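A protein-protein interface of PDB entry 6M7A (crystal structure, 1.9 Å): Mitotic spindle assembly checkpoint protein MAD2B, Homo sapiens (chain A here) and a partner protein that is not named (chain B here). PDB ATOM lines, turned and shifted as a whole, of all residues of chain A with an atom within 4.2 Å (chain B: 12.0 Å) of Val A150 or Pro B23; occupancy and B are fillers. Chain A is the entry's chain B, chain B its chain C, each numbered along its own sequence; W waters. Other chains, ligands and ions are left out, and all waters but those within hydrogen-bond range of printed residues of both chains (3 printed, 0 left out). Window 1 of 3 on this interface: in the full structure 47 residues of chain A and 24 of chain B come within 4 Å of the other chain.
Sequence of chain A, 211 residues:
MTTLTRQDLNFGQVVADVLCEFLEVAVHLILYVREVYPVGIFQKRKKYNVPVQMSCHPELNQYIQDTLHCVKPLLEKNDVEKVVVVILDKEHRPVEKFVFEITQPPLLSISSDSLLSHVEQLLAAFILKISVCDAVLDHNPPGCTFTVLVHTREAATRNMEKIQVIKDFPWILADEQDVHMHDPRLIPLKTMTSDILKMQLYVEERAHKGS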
ATOM      1  N   VAL A  71       0.954   4.388  16.724  1.00  0.00           N
ATOM      2  CA  VAL A  71       0.974   2.971  17.070  1.00  0.00           C
ATOM      3  C   VAL A  71       2.164   2.638  17.972  1.00  0.00           C
ATOM      4  O   VAL A  71       2.080   1.740  18.820  1.00  0.00           O
ATOM      5  CB  VAL A  71       0.983   2.112  15.789  1.00  0.00           C
ATOM      6  CG1 VAL A  71       0.935   0.637  16.146  1.00  0.00           C
ATOM      7  CG2 VAL A  71      -0.203   2.471  14.896  1.00  0.00           C
ATOM      8  N   LYS A  82      -2.951  -6.779  15.789  1.00  0.00           N
ATOM      9  CA  LYS A  82      -2.856  -6.675  14.340  1.00  0.00           C
ATOM     10  C   LYS A  82      -2.722  -5.215  13.935  1.00  0.00           C
ATOM     11  O   LYS A  82      -3.361  -4.340  14.527  1.00  0.00           O
ATOM     12  CB  LYS A  82      -4.103  -7.252  13.619  1.00  0.00           C
ATOM     13  CG  LYS A  82      -4.610  -8.568  14.148  1.00  0.00           C
ATOM     14  CD  LYS A  82      -5.497  -9.288  13.151  1.00  0.00           C
ATOM     15  CE  LYS A  82      -6.906  -8.725  13.124  1.00  0.00           C
ATOM     16  NZ  LYS A  82      -7.942  -9.757  13.439  1.00  0.00           N
ATOM     17  N   LEU A 149      -5.769   0.100  10.106  1.00  0.00           N
ATOM     18  CA  LEU A 149      -6.544  -0.335  11.266  1.00  0.00           C
ATOM     19  C   LEU A 149      -5.599  -0.906  12.305  1.00  0.00           C
ATOM     20  O   LEU A 149      -4.652  -1.629  11.964  1.00  0.00           O
ATOM     21  CB  LEU A 149      -7.579  -1.420  10.904  1.00  0.00           C
ATOM     22  CG  LEU A 149      -8.516  -1.190   9.727  1.00  0.00           C
ATOM     23  CD1 LEU A 149      -9.398  -2.424   9.499  1.00  0.00           C
ATOM     24  CD2 LEU A 149      -9.359   0.026   9.987  1.00  0.00           C
ATOM     25  N   VAL A 150      -5.853  -0.598  13.567  1.00  0.00           N
ATOM     26  CA  VAL A 150      -5.039  -1.113  14.665  1.00  0.00           C
ATOM     27  C   VAL A 150      -5.948  -1.904  15.596  1.00  0.00           C
ATOM     28  O   VAL A 150      -6.848  -1.333  16.222  1.00  0.00           O
ATOM     29  CB  VAL A 150      -4.319   0.015  15.416  1.00  0.00           C
ATOM     30  CG1 VAL A 150      -3.551  -0.541  16.609  1.00  0.00           C
ATOM     31  CG2 VAL A 150      -3.383   0.799  14.460  1.00  0.00           C
ATOM     32  N   HIS A 151      -5.708  -3.211  15.685  1.00  0.00           N
ATOM     33  CA  HIS A 151      -6.472  -4.107  16.545  1.00  0.00           C
ATOM     34  C   HIS A 151      -5.700  -4.299  17.847  1.00  0.00           C
ATOM     35  O   HIS A 151      -4.574  -4.813  17.832  1.00  0.00           O
ATOM     36  CB  HIS A 151      -6.709  -5.446  15.846  1.00  0.00           C
ATOM     37  CG  HIS A 151      -7.594  -5.349  14.643  1.00  0.00           C
ATOM     38  ND1 HIS A 151      -8.930  -5.683  14.677  1.00  0.00           N
ATOM     39  CD2 HIS A 151      -7.340  -4.942  13.375  1.00  0.00           C
ATOM     40  CE1 HIS A 151      -9.461  -5.500  13.481  1.00  0.00           C
ATOM     41  NE2 HIS A 151      -8.521  -5.043  12.674  1.00  0.00           N
ATOM     42  N   THR A 152      -6.299  -3.875  18.961  1.00  0.00           N
ATOM     43  CA  THR A 152      -5.657  -3.894  20.268  1.00  0.00           C
ATOM     44  C   THR A 152      -5.965  -5.194  20.998  1.00  0.00           C
ATOM     45  O   THR A 152      -6.926  -5.902  20.685  1.00  0.00           O
ATOM     46  CB  THR A 152      -6.125  -2.710  21.118  1.00  0.00           C
ATOM     47  OG1 THR A 152      -7.549  -2.765  21.257  1.00  0.00           O
ATOM     48  CG2 THR A 152      -5.752  -1.402  20.458  1.00  0.00           C
ATOM     49  N   TRP A 171      -7.903   9.728  16.219  1.00  0.00           N
ATOM     50  CA  TRP A 171      -8.300   8.382  15.829  1.00  0.00           C
ATOM     51  C   TRP A 171      -9.752   8.152  16.221  1.00  0.00           C
ATOM     52  O   TRP A 171     -10.280   8.797  17.129  1.00  0.00           O
ATOM     53  CB  TRP A 171      -7.426   7.318  16.504  1.00  0.00           C
ATOM     54  CG  TRP A 171      -6.033   7.255  15.960  1.00  0.00           C
ATOM     55  CD1 TRP A 171      -5.065   8.226  16.050  1.00  0.00           C
ATOM     56  CD2 TRP A 171      -5.438   6.164  15.251  1.00  0.00           C
ATOM     57  NE1 TRP A 171      -3.910   7.803  15.435  1.00  0.00           N
ATOM     58  CE2 TRP A 171      -4.110   6.540  14.941  1.00  0.00           C
ATOM     59  CE3 TRP A 171      -5.889   4.900  14.861  1.00  0.00           C
ATOM     60  CZ2 TRP A 171      -3.238   5.694  14.261  1.00  0.00           C
ATOM     61  CZ3 TRP A 171      -5.021   4.068  14.160  1.00  0.00           C
ATOM     62  CH2 TRP A 171      -3.715   4.466  13.872  1.00  0.00           C
ATOM     63  N   LEU A 173     -12.882   4.811  16.567  1.00  0.00           N
ATOM     64  CA  LEU A 173     -13.313   3.433  16.383  1.00  0.00           C
ATOM     65  C   LEU A 173     -13.712   3.216  14.933  1.00  0.00           C
ATOM     66  O   LEU A 173     -14.473   4.003  14.365  1.00  0.00           O
ATOM     67  CB  LEU A 173     -14.502   3.138  17.296  1.00  0.00           C
ATOM     68  CG  LEU A 173     -14.206   2.631  18.700  1.00  0.00           C
ATOM     69  CD1 LEU A 173     -15.514   2.353  19.404  1.00  0.00           C
ATOM     70  CD2 LEU A 173     -13.349   1.381  18.632  1.00  0.00           C
ATOM     71  N   ALA A 174     -13.205   2.152  14.329  1.00  0.00           N
ATOM     72  CA  ALA A 174     -13.614   1.845  12.969  1.00  0.00           C
ATOM     73  C   ALA A 174     -15.063   1.357  12.944  1.00  0.00           C
ATOM     74  O   ALA A 174     -15.578   0.814  13.927  1.00  0.00           O
ATOM     75  CB  ALA A 174     -12.673   0.801  12.358  1.00  0.00           C
ATOM     76  N   VAL A 179     -13.994  -2.745   7.986  1.00  0.00           N
ATOM     77  CA  VAL A 179     -13.183  -3.862   8.452  1.00  0.00           C
ATOM     78  C   VAL A 179     -13.646  -5.177   7.843  1.00  0.00           C
ATOM     79  O   VAL A 179     -12.833  -5.974   7.360  1.00  0.00           O
ATOM     80  CB  VAL A 179     -13.195  -3.951   9.999  1.00  0.00           C
ATOM     81  CG1 VAL A 179     -12.334  -5.120  10.497  1.00  0.00           C
ATOM     82  CG2 VAL A 179     -12.749  -2.633  10.616  1.00  0.00           C
ATOM     83  N   PHE B  15      -5.320 -14.369  14.865  1.00  0.00           N
ATOM     84  CA  PHE B  15      -6.352 -13.481  15.400  1.00  0.00           C
ATOM     85  C   PHE B  15      -7.477 -13.346  14.378  1.00  0.00           C
ATOM     86  O   PHE B  15      -7.561 -12.340  13.659  1.00  0.00           O
ATOM     87  CB  PHE B  15      -5.768 -12.105  15.736  1.00  0.00           C
ATOM     88  CG  PHE B  15      -4.590 -12.146  16.680  1.00  0.00           C
ATOM     89  CD1 PHE B  15      -4.763 -12.522  18.003  1.00  0.00           C
ATOM     90  CD2 PHE B  15      -3.321 -11.796  16.245  1.00  0.00           C
ATOM     91  CE1 PHE B  15      -3.683 -12.556  18.881  1.00  0.00           C
ATOM     92  CE2 PHE B  15      -2.232 -11.827  17.116  1.00  0.00           C
ATOM     93  CZ  PHE B  15      -2.415 -12.206  18.436  1.00  0.00           C
ATOM     94  N   PRO B  16      -8.366 -14.334  14.290  1.00  0.00           N
ATOM     95  CA  PRO B  16      -9.462 -14.249  13.314  1.00  0.00           C
ATOM     96  C   PRO B  16     -10.351 -13.039  13.580  1.00  0.00           C
ATOM     97  O   PRO B  16     -10.445 -12.547  14.707  1.00  0.00           O
ATOM     98  CB  PRO B  16     -10.225 -15.559  13.525  1.00  0.00           C
ATOM     99  CG  PRO B  16      -9.942 -15.924  14.951  1.00  0.00           C
ATOM    100  CD  PRO B  16      -8.543 -15.451  15.238  1.00  0.00           C
ATOM    101  N   TYR B  17     -10.995 -12.551  12.520  1.00  0.00           N
ATOM    102  CA  TYR B  17     -11.861 -11.380  12.640  1.00  0.00           C
ATOM    103  C   TYR B  17     -12.901 -11.591  13.733  1.00  0.00           C
ATOM    104  O   TYR B  17     -13.627 -12.593  13.746  1.00  0.00           O
ATOM    105  CB  TYR B  17     -12.550 -11.071  11.301  1.00  0.00           C
ATOM    106  CG  TYR B  17     -13.710 -10.097  11.426  1.00  0.00           C
ATOM    107  CD1 TYR B  17     -15.000 -10.549  11.716  1.00  0.00           C
ATOM    108  CD2 TYR B  17     -13.517  -8.730  11.260  1.00  0.00           C
ATOM    109  CE1 TYR B  17     -16.058  -9.664  11.852  1.00  0.00           C
ATOM    110  CE2 TYR B  17     -14.575  -7.836  11.390  1.00  0.00           C
ATOM    111  CZ  TYR B  17     -15.841  -8.308  11.684  1.00  0.00           C
ATOM    112  OH  TYR B  17     -16.895  -7.425  11.806  1.00  0.00           O
ATOM    113  N   ASP B  18     -12.978 -10.634  14.650  1.00  0.00           N
ATOM    114  CA  ASP B  18     -13.904 -10.704  15.781  1.00  0.00           C
ATOM    115  C   ASP B  18     -14.684  -9.394  15.826  1.00  0.00           C
ATOM    116  O   ASP B  18     -14.156  -8.369  16.269  1.00  0.00           O
ATOM    117  CB  ASP B  18     -13.143 -10.964  17.078  1.00  0.00           C
ATOM    118  CG  ASP B  18     -14.024 -10.865  18.322  1.00  0.00           C
ATOM    119  OD1 ASP B  18     -15.264 -10.845  18.192  1.00  0.00           O
ATOM    120  OD2 ASP B  18     -13.462 -10.829  19.441  1.00  0.00           O
ATOM    121  N   GLY B  19     -15.939  -9.429  15.384  1.00  0.00           N
ATOM    122  CA  GLY B  19     -16.760  -8.230  15.330  1.00  0.00           C
ATOM    123  C   GLY B  19     -17.088  -7.619  16.679  1.00  0.00           C
ATOM    124  O   GLY B  19     -17.585  -6.487  16.711  1.00  0.00           O
ATOM    125  N   SER B  20     -16.819  -8.332  17.783  1.00  0.00           N
ATOM    126  CA  SER B  20     -17.074  -7.820  19.127  1.00  0.00           C
ATOM    127  C   SER B  20     -16.015  -6.840  19.614  1.00  0.00           C
ATOM    128  O   SER B  20     -16.243  -6.165  20.627  1.00  0.00           O
ATOM    129  CB  SER B  20     -17.176  -8.980  20.128  1.00  0.00           C
ATOM    130  OG  SER B  20     -15.881  -9.444  20.477  1.00  0.00           O
ATOM    131  N   LYS B  21     -14.862  -6.752  18.946  1.00  0.00           N
ATOM    132  CA  LYS B  21     -13.840  -5.757  19.279  1.00  0.00           C
ATOM    133  C   LYS B  21     -13.357  -5.081  17.996  1.00  0.00           C
ATOM    134  O   LYS B  21     -12.502  -5.613  17.279  1.00  0.00           O
ATOM    135  CB  LYS B  21     -12.680  -6.377  20.040  1.00  0.00           C
ATOM    136  CG  LYS B  21     -11.678  -5.329  20.499  1.00  0.00           C
ATOM    137  CD  LYS B  21     -10.825  -5.847  21.624  1.00  0.00           C
ATOM    138  CE  LYS B  21     -10.371  -7.258  21.341  1.00  0.00           C
ATOM    139  NZ  LYS B  21      -8.909  -7.408  21.597  1.00  0.00           N
ATOM    140  N   LEU B  22     -13.895  -3.904  17.722  1.00  0.00           N
ATOM    141  CA  LEU B  22     -13.574  -3.143  16.529  1.00  0.00           C
ATOM    142  C   LEU B  22     -12.193  -2.516  16.681  1.00  0.00           C
ATOM    143  O   LEU B  22     -11.761  -2.228  17.795  1.00  0.00           O
ATOM    144  CB  LEU B  22     -14.615  -2.046  16.295  1.00  0.00           C
ATOM    145  CG  LEU B  22     -16.027  -2.463  15.881  1.00  0.00           C
ATOM    146  CD1 LEU B  22     -16.988  -1.287  16.000  1.00  0.00           C
ATOM    147  CD2 LEU B  22     -16.032  -3.014  14.461  1.00  0.00           C
ATOM    148  N   PRO B  23     -11.480  -2.309  15.585  1.00  0.00           N
ATOM    149  CA  PRO B  23     -10.154  -1.700  15.656  1.00  0.00           C
ATOM    150  C   PRO B  23     -10.258  -0.179  15.648  1.00  0.00           C
ATOM    151  O   PRO B  23     -11.323   0.396  15.426  1.00  0.00           O
ATOM    152  CB  PRO B  23      -9.480  -2.202  14.376  1.00  0.00           C
ATOM    153  CG  PRO B  23     -10.614  -2.224  13.404  1.00  0.00           C
ATOM    154  CD  PRO B  23     -11.820  -2.709  14.204  1.00  0.00           C
ATOM    155  N   LEU B  24      -9.119   0.456  15.899  1.00  0.00           N
ATOM    156  CA  LEU B  24      -8.964   1.898  15.781  1.00  0.00           C
ATOM    157  C   LEU B  24      -8.456   2.234  14.389  1.00  0.00           C
ATOM    158  O   LEU B  24      -7.706   1.461  13.790  1.00  0.00           O
ATOM    159  CB  LEU B  24      -7.965   2.422  16.820  1.00  0.00           C
ATOM    160  CG  LEU B  24      -8.226   1.991  18.262  1.00  0.00           C
ATOM    161  CD1 LEU B  24      -7.113   2.391  19.191  1.00  0.00           C
ATOM    162  CD2 LEU B  24      -9.485   2.656  18.675  1.00  0.00           C
ATOM    163  N   ARG B  25      -8.854   3.394  13.884  1.00  0.00           N
ATOM    164  CA  ARG B  25      -8.326   3.903  12.627  1.00  0.00           C
ATOM    165  C   ARG B  25      -8.210   5.418  12.712  1.00  0.00           C
ATOM    166  O   ARG B  25      -8.894   6.055  13.521  1.00  0.00           O
ATOM    167  CB  ARG B  25      -9.197   3.492  11.434  1.00  0.00           C
ATOM    168  CG  ARG B  25     -10.418   4.342  11.196  1.00  0.00           C
ATOM    169  CD  ARG B  25     -11.083   3.941   9.879  1.00  0.00           C
ATOM    170  NE  ARG B  25     -12.452   4.433   9.779  1.00  0.00           N
ATOM    171  CZ  ARG B  25     -12.774   5.693   9.498  1.00  0.00           C
ATOM    172  NH1 ARG B  25     -14.047   6.055   9.424  1.00  0.00           N
ATOM    173  NH2 ARG B  25     -11.819   6.592   9.281  1.00  0.00           N
ATOM    174  N   PRO B  26      -7.314   6.017  11.927  1.00  0.00           N
ATOM    175  CA  PRO B  26      -7.227   7.485  11.917  1.00  0.00           C
ATOM    176  C   PRO B  26      -8.535   8.078  11.409  1.00  0.00           C
ATOM    177  O   PRO B  26      -9.194   7.509  10.540  1.00  0.00           O
ATOM    178  CB  PRO B  26      -6.061   7.775  10.959  1.00  0.00           C
ATOM    179  CG  PRO B  26      -5.260   6.475  10.898  1.00  0.00           C
ATOM    180  CD  PRO B  26      -6.309   5.391  11.039  1.00  0.00           C
ATOM    181  N   LYS B  27      -8.927   9.213  11.989  1.00  0.00           N
ATOM    182  CA  LYS B  27     -10.186   9.840  11.585  1.00  0.00           C
ATOM    183  C   LYS B  27     -10.063  10.478  10.212  1.00  0.00           C
ATOM    184  O   LYS B  27     -10.994  10.418   9.405  1.00  0.00           O
ATOM    185  CB  LYS B  27     -10.610  10.886  12.621  1.00  0.00           C
ATOM    186  CG  LYS B  27     -11.962  11.545  12.314  1.00  0.00           C
ATOM    187  CD  LYS B  27     -12.405  12.423  13.480  1.00  0.00           C
ATOM    188  CE  LYS B  27     -13.708  13.164  13.182  1.00  0.00           C
ATOM    189  NZ  LYS B  27     -14.158  13.877  14.419  1.00  0.00           N
ATOM    190  N   ARG B  28      -8.930  11.114   9.942  1.00  0.00           N
ATOM    191  CA  ARG B  28      -8.690  11.715   8.643  1.00  0.00           C
ATOM    192  C   ARG B  28      -8.225  10.656   7.655  1.00  0.00           C
ATOM    193  O   ARG B  28      -7.543   9.696   8.021  1.00  0.00           O
ATOM    194  CB  ARG B  28      -7.637  12.820   8.747  1.00  0.00           C
ATOM    195  CG  ARG B  28      -7.926  13.868   9.806  1.00  0.00           C
ATOM    196  CD  ARG B  28      -6.610  14.408  10.371  1.00  0.00           C
ATOM    197  NE  ARG B  28      -5.557  14.363   9.358  1.00  0.00           N
ATOM    198  CZ  ARG B  28      -4.302  14.758   9.552  1.00  0.00           C
ATOM    199  NH1 ARG B  28      -3.929  15.239  10.730  1.00  0.00           N
ATOM    200  NH2 ARG B  28      -3.419  14.671   8.564  1.00  0.00           N
HETATM  201  O   HOH W   1     -10.094  -9.295  14.975  1.00  0.00           O
HETATM  202  O   HOH W   2     -10.176  -6.407  17.144  1.00  0.00           O
HETATM  203  O   HOH W   3      -9.142  -3.925  18.750  1.00  0.00           O
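The backbone carbonyl oxygen (O) of Lys A82 sits at hydrogen-bond distance from the backbone NH (N) of His A151.
Of chain B, only Pro B23 (3.3 Å) and Leu B24 (2.8 Å) come within 4 Å of Val A150. Printed residues of chain A within 4 Å of Pro B23: Val A150 (3.3 Å), His A151 (3.4 Å), Leu A173 (3.7 Å), Ala A174 (2.8 Å) and Val A179 (3.5 Å). No residue of chain B comes within 4 Å of Val A71. Lys A82 touches just these residues of chain B: Phe B15 (2.6 Å) and Pro B16 (3.96 Å). His A151 touches just one residue of chain B: Pro B23 (3.4 Å). Of chain B, only Lys B21 comes within 4 Å of Thr A152. Of chain B, only Pro B23 comes within 4 Å of Leu A173. Ala A174 touches just these residues of chain B: Leu B22 (3.3 Å) and Pro B23 (2.8 Å). Of the printed residues of chain A, Tyr B17 touches Val A179 (3.6 Å). Printed residues of chain A within 4 Å of Lys B21: Thr A152 (2.7 Å). Printed residues of chain A within 4 Å of Lys B27: Trp A171. Printed residues of chain A within 4 Å of Leu B22: Ala A174 (3.3 Å). Arg B28 touches none of the printed residues of chain A. The nearest residue of chain B that does not touch Val A150 is Arg B25 (5.0 Å). The nearest printed residue of chain A that does not touch Pro B26 is Leu A149 (5.4 Å).
Lys A82 touches Pro B16 (NZ to O, 3.96 Å). Leu A149 touches Leu B24. Arg B25 touches Leu A149. Pro B23 touches Val A150 (CB to O, 3.3 Å). Arg B25 touches Trp A171 (C to CE3, 3.2 Å). Pro B26 touches Trp A171 (N to CE3, 3.4 Å). CA of Trp A171 touches N of Lys B27 (3.98 Å). Leu A173 touches Pro B23. Tyr B17 touches Val A179 (CE2 to CG1, 3.6 Å). CG2 of Val A179 touches CG of Pro B23, 3.5 Å away.
The backbone NH (N) of Ala A174 lies within hydrogen-bond range of the backbone carbonyl oxygen (O) of Pro B23 (2.8 Å). N of Val A150 sits at hydrogen-bond distance from O of Leu B24 (2.8 Å). The side-chain amino group (NZ) of Lys A82 is in hydrogen-bond range of the backbone carbonyl oxygen (O) of Phe B15 (2.6 Å). NZ of Lys B21 lies within hydrogen-bond range of O of Thr A152 (2.7 Å).
Printed residues of chain B that touch a printed residue of chain A: Phe B15, Pro B16, Tyr B17, Lys B21, Leu B22, Pro B23, Leu B24, Arg B25, Pro B26 and Lys B27. Hydrophobic or aromatic side chains of chain B within 4 Å of the printed part of chain A: Phe B15, Tyr B17, Leu B22, Pro B23, Leu B24 and Pro B26. Along chain B the printed residues that touch a printed residue of chain A span positions 15 to 27. Of the 10 printed residues of chain A, 9 touch a printed residue of chain B. Among the printed residues, 17 pairs touch across the chains.
Water W2 bridges the backbone carbonyl oxygen (O) of Lys B21 and a ring nitrogen (ND1) of His A151. Water W1 lies within hydrogen-bond range of the side-chain amino group (NZ) of Lys A82 (2.7 Å), the backbone NH (N) of Asp B18 (3.2 Å) and the backbone carbonyl oxygen (O) of Pro B16 (3.3 Å). Water W3 bridges the backbone NH (N) of Thr A152 and the backbone carbonyl oxygen (O) of Leu B22.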
